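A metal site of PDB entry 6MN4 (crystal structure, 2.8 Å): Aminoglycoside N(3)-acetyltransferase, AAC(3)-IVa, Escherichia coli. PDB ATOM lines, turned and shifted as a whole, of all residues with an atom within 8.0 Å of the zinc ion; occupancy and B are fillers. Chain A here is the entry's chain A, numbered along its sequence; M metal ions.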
ATOM      1  N   HIS A 190      13.162 -22.554   0.688  1.00  0.00           N
ATOM      2  CA  HIS A 190      11.858 -22.852   0.117  1.00  0.00           C
ATOM      3  C   HIS A 190      11.546 -21.765  -0.910  1.00  0.00           C
ATOM      4  O   HIS A 190      12.458 -21.066  -1.378  1.00  0.00           O
ATOM      5  CB  HIS A 190      10.805 -22.960   1.226  1.00  0.00           C
ATOM      6  CG  HIS A 190      11.059 -22.064   2.394  1.00  0.00           C
ATOM      7  ND1 HIS A 190      10.898 -20.696   2.333  1.00  0.00           N
ATOM      8  CD2 HIS A 190      11.485 -22.334   3.645  1.00  0.00           C
ATOM      9  CE1 HIS A 190      11.203 -20.166   3.502  1.00  0.00           C
ATOM     10  NE2 HIS A 190      11.568 -21.138   4.316  1.00  0.00           N
ATOM     11  N   CYS A 191      10.272 -21.612  -1.243  1.00  0.00           N
ATOM     12  CA  CYS A 191       9.876 -20.584  -2.194  1.00  0.00           C
ATOM     13  C   CYS A 191      10.160 -19.169  -1.681  1.00  0.00           C
ATOM     14  O   CYS A 191      10.293 -18.248  -2.484  1.00  0.00           O
ATOM     15  CB  CYS A 191       8.393 -20.733  -2.538  1.00  0.00           C
ATOM     16  SG  CYS A 191       7.249 -20.354  -1.208  1.00  0.00           S
ATOM     17  N   CYS A 192      10.262 -19.000  -0.363  1.00  0.00           N
ATOM     18  CA  CYS A 192      10.523 -17.720   0.291  1.00  0.00           C
ATOM     19  C   CYS A 192       9.424 -16.692   0.043  1.00  0.00           C
ATOM     20  O   CYS A 192       9.592 -15.527   0.413  1.00  0.00           O
ATOM     21  CB  CYS A 192      11.885 -17.146  -0.111  1.00  0.00           C
ATOM     22  SG  CYS A 192      13.311 -17.991   0.605  1.00  0.00           S
ATOM     23  N   GLU A 193       8.315 -17.099  -0.585  1.00  0.00           N
ATOM     24  CA  GLU A 193       7.232 -16.154  -0.849  1.00  0.00           C
ATOM     25  C   GLU A 193       6.642 -15.631   0.454  1.00  0.00           C
ATOM     26  O   GLU A 193       6.397 -14.431   0.593  1.00  0.00           O
ATOM     27  CB  GLU A 193       6.158 -16.826  -1.699  1.00  0.00           C
ATOM     28  CG  GLU A 193       6.531 -16.992  -3.164  1.00  0.00           C
ATOM     29  CD  GLU A 193       5.376 -17.496  -4.013  1.00  0.00           C
ATOM     30  OE1 GLU A 193       4.218 -17.463  -3.531  1.00  0.00           O
ATOM     31  OE2 GLU A 193       5.620 -17.935  -5.155  1.00  0.00           O
ATOM     32  N   ARG A 194       6.416 -16.511   1.420  1.00  0.00           N
ATOM     33  CA  ARG A 194       5.809 -16.117   2.683  1.00  0.00           C
ATOM     34  C   ARG A 194       6.748 -15.299   3.567  1.00  0.00           C
ATOM     35  O   ARG A 194       6.359 -14.953   4.696  1.00  0.00           O
ATOM     36  CB  ARG A 194       5.323 -17.347   3.443  1.00  0.00           C
ATOM     37  CG  ARG A 194       4.120 -18.016   2.806  1.00  0.00           C
ATOM     38  CD  ARG A 194       3.750 -19.300   3.512  1.00  0.00           C
ATOM     39  NE  ARG A 194       3.326 -19.073   4.890  1.00  0.00           N
ATOM     40  CZ  ARG A 194       2.080 -18.794   5.245  1.00  0.00           C
ATOM     41  NH1 ARG A 194       1.130 -18.728   4.329  1.00  0.00           N
ATOM     42  NH2 ARG A 194       1.783 -18.598   6.522  1.00  0.00           N
ATOM     43  N   PHE A 241       6.653 -19.801   7.555  1.00  0.00           N
ATOM     44  CA  PHE A 241       7.193 -19.435   6.258  1.00  0.00           C
ATOM     45  C   PHE A 241       6.950 -20.510   5.200  1.00  0.00           C
ATOM     46  O   PHE A 241       7.268 -20.299   4.030  1.00  0.00           O
ATOM     47  CB  PHE A 241       8.693 -19.151   6.359  1.00  0.00           C
ATOM     48  CG  PHE A 241       9.010 -17.874   7.085  1.00  0.00           C
ATOM     49  CD1 PHE A 241       8.173 -16.775   6.992  1.00  0.00           C
ATOM     50  CD2 PHE A 241      10.159 -17.770   7.863  1.00  0.00           C
ATOM     51  CE1 PHE A 241       8.458 -15.601   7.664  1.00  0.00           C
ATOM     52  CE2 PHE A 241      10.452 -16.601   8.539  1.00  0.00           C
ATOM     53  CZ  PHE A 241       9.600 -15.513   8.433  1.00  0.00           C
ATOM     54  N   LEU A 242       6.396 -21.659   5.596  1.00  0.00           N
ATOM     55  CA  LEU A 242       6.090 -22.730   4.660  1.00  0.00           C
ATOM     56  C   LEU A 242       4.682 -22.555   4.111  1.00  0.00           C
ATOM     57  O   LEU A 242       3.748 -22.232   4.843  1.00  0.00           O
ATOM     58  CB  LEU A 242       6.209 -24.092   5.325  1.00  0.00           C
ATOM     59  CG  LEU A 242       7.574 -24.554   5.828  1.00  0.00           C
ATOM     60  CD1 LEU A 242       7.551 -26.064   6.007  1.00  0.00           C
ATOM     61  CD2 LEU A 242       8.698 -24.117   4.883  1.00  0.00           C
ATOM     62  N   HIS A 243       4.545 -22.784   2.813  1.00  0.00           N
ATOM     63  CA  HIS A 243       3.229 -22.828   2.217  1.00  0.00           C
ATOM     64  C   HIS A 243       2.474 -24.051   2.755  1.00  0.00           C
ATOM     65  O   HIS A 243       3.061 -25.114   2.919  1.00  0.00           O
ATOM     66  CB  HIS A 243       3.332 -22.899   0.694  1.00  0.00           C
ATOM     67  CG  HIS A 243       3.402 -21.557   0.034  1.00  0.00           C
ATOM     68  ND1 HIS A 243       4.166 -21.313  -1.084  1.00  0.00           N
ATOM     69  CD2 HIS A 243       2.788 -20.385   0.332  1.00  0.00           C
ATOM     70  CE1 HIS A 243       4.012 -20.054  -1.446  1.00  0.00           C
ATOM     71  NE2 HIS A 243       3.195 -19.463  -0.602  1.00  0.00           N
ATOM     72  N   PRO A 244       1.184 -23.915   3.048  1.00  0.00           N
ATOM     73  CA  PRO A 244       0.399 -25.082   3.449  1.00  0.00           C
ATOM     74  C   PRO A 244       0.279 -26.053   2.295  1.00  0.00           C
ATOM     75  O   PRO A 244       0.410 -25.665   1.122  1.00  0.00           O
ATOM     76  CB  PRO A 244      -0.958 -24.475   3.825  1.00  0.00           C
ATOM     77  CG  PRO A 244      -1.023 -23.183   3.073  1.00  0.00           C
ATOM     78  CD  PRO A 244       0.390 -22.675   3.042  1.00  0.00           C
ATOM     79  N   ALA A 247      -1.820 -25.038  -0.753  1.00  0.00           N
ATOM     80  CA  ALA A 247      -1.305 -24.165  -1.805  1.00  0.00           C
ATOM     81  C   ALA A 247      -0.571 -24.940  -2.886  1.00  0.00           C
ATOM     82  O   ALA A 247      -0.359 -24.397  -3.981  1.00  0.00           O
ATOM     83  CB  ALA A 247      -0.401 -23.091  -1.209  1.00  0.00           C
ATOM     84  N   GLY A 248      -0.159 -26.172  -2.606  1.00  0.00           N
ATOM     85  CA  GLY A 248       0.505 -26.991  -3.623  1.00  0.00           C
ATOM     86  C   GLY A 248       1.836 -26.451  -4.092  1.00  0.00           C
ATOM     87  O   GLY A 248       2.146 -26.561  -5.296  1.00  0.00           O
ATOM     88  N   CYS A 249       2.624 -25.872  -3.198  1.00  0.00           N
ATOM     89  CA  CYS A 249       3.950 -25.354  -3.542  1.00  0.00           C
ATOM     90  C   CYS A 249       4.962 -26.484  -3.457  1.00  0.00           C
ATOM     91  O   CYS A 249       5.247 -27.001  -2.377  1.00  0.00           O
ATOM     92  CB  CYS A 249       4.317 -24.210  -2.605  1.00  0.00           C
ATOM     93  SG  CYS A 249       6.082 -23.753  -2.585  1.00  0.00           S
ATOM     94  N   GLU A 250       5.509 -26.863  -4.619  1.00  0.00           N
ATOM     95  CA  GLU A 250       6.467 -27.974  -4.675  1.00  0.00           C
ATOM     96  C   GLU A 250       7.683 -27.707  -3.801  1.00  0.00           C
ATOM     97  O   GLU A 250       8.252 -28.647  -3.227  1.00  0.00           O
ATOM     98  CB  GLU A 250       6.884 -28.218  -6.124  1.00  0.00           C
ATOM     99  CG  GLU A 250       7.256 -29.666  -6.433  1.00  0.00           C
ATOM    100  CD  GLU A 250       6.876 -30.075  -7.859  1.00  0.00           C
ATOM    101  OE1 GLU A 250       5.674 -30.318  -8.112  1.00  0.00           O
ATOM    102  OE2 GLU A 250       7.771 -30.136  -8.717  1.00  0.00           O
ATOM    103  N   GLU A 251       8.100 -26.448  -3.682  1.00  0.00           N
ATOM    104  CA  GLU A 251       9.289 -26.137  -2.885  1.00  0.00           C
ATOM    105  C   GLU A 251       9.017 -26.305  -1.401  1.00  0.00           C
ATOM    106  O   GLU A 251       9.803 -26.917  -0.679  1.00  0.00           O
ATOM    107  CB  GLU A 251       9.758 -24.718  -3.200  1.00  0.00           C
ATOM    108  CG  GLU A 251      11.265 -24.525  -3.137  1.00  0.00           C
ATOM    109  CD  GLU A 251      11.752 -23.407  -4.042  1.00  0.00           C
ATOM    110  OE1 GLU A 251      12.961 -23.108  -4.014  1.00  0.00           O
ATOM    111  OE2 GLU A 251      10.922 -22.831  -4.778  1.00  0.00           O
ATOM    112  N   CYS A 252       7.895 -25.764  -0.930  1.00  0.00           N
ATOM    113  CA  CYS A 252       7.592 -25.824   0.496  1.00  0.00           C
ATOM    114  C   CYS A 252       7.207 -27.241   0.915  1.00  0.00           C
ATOM    115  O   CYS A 252       7.545 -27.682   2.018  1.00  0.00           O
ATOM    116  CB  CYS A 252       6.463 -24.844   0.831  1.00  0.00           C
ATOM    117  SG  CYS A 252       6.987 -23.120   0.797  1.00  0.00           S
ATOM    118  N   ASP A 253       6.483 -27.957   0.044  1.00  0.00           N
ATOM    119  CA  ASP A 253       6.108 -29.330   0.360  1.00  0.00           C
ATOM    120  C   ASP A 253       7.322 -30.209   0.570  1.00  0.00           C
ATOM    121  O   ASP A 253       7.288 -31.151   1.381  1.00  0.00           O
ATOM    122  CB  ASP A 253       5.219 -29.897  -0.756  1.00  0.00           C
ATOM    123  CG  ASP A 253       3.826 -29.301  -0.753  1.00  0.00           C
ATOM    124  OD1 ASP A 253       3.529 -28.464   0.125  1.00  0.00           O
ATOM    125  OD2 ASP A 253       3.020 -29.684  -1.632  1.00  0.00           O
HETATM  126 ZN    ZN M   1       6.131 -22.180  -1.024  1.00  0.00          ZN
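The side-chain sulfur (SG) of Cys 191 lies close to the backbone NH (N) of Glu 193, at 3.5 Å.
The side-chain sulfur (SG) of Cys 249 lies close to the backbone NH (N) of Glu 251 (3.5 Å).
Four residues have an atom within 4 Å of the zinc ion: Cys 191, His 243, Cys 249 and Cys 252.
Along chain A the residues within 4 Å of the zinc ion span positions 191 to 252.
The zinc ion is bound by the side-chain sulfur (SG) of Cys 191, at 2.1 Å.
ND1 of His 243 is bound to the zinc ion.
The zinc ion is bound by SG of Cys 249 (2.2 Å).
The zinc ion is bound by SG of Cys 252, at 2.2 Å.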
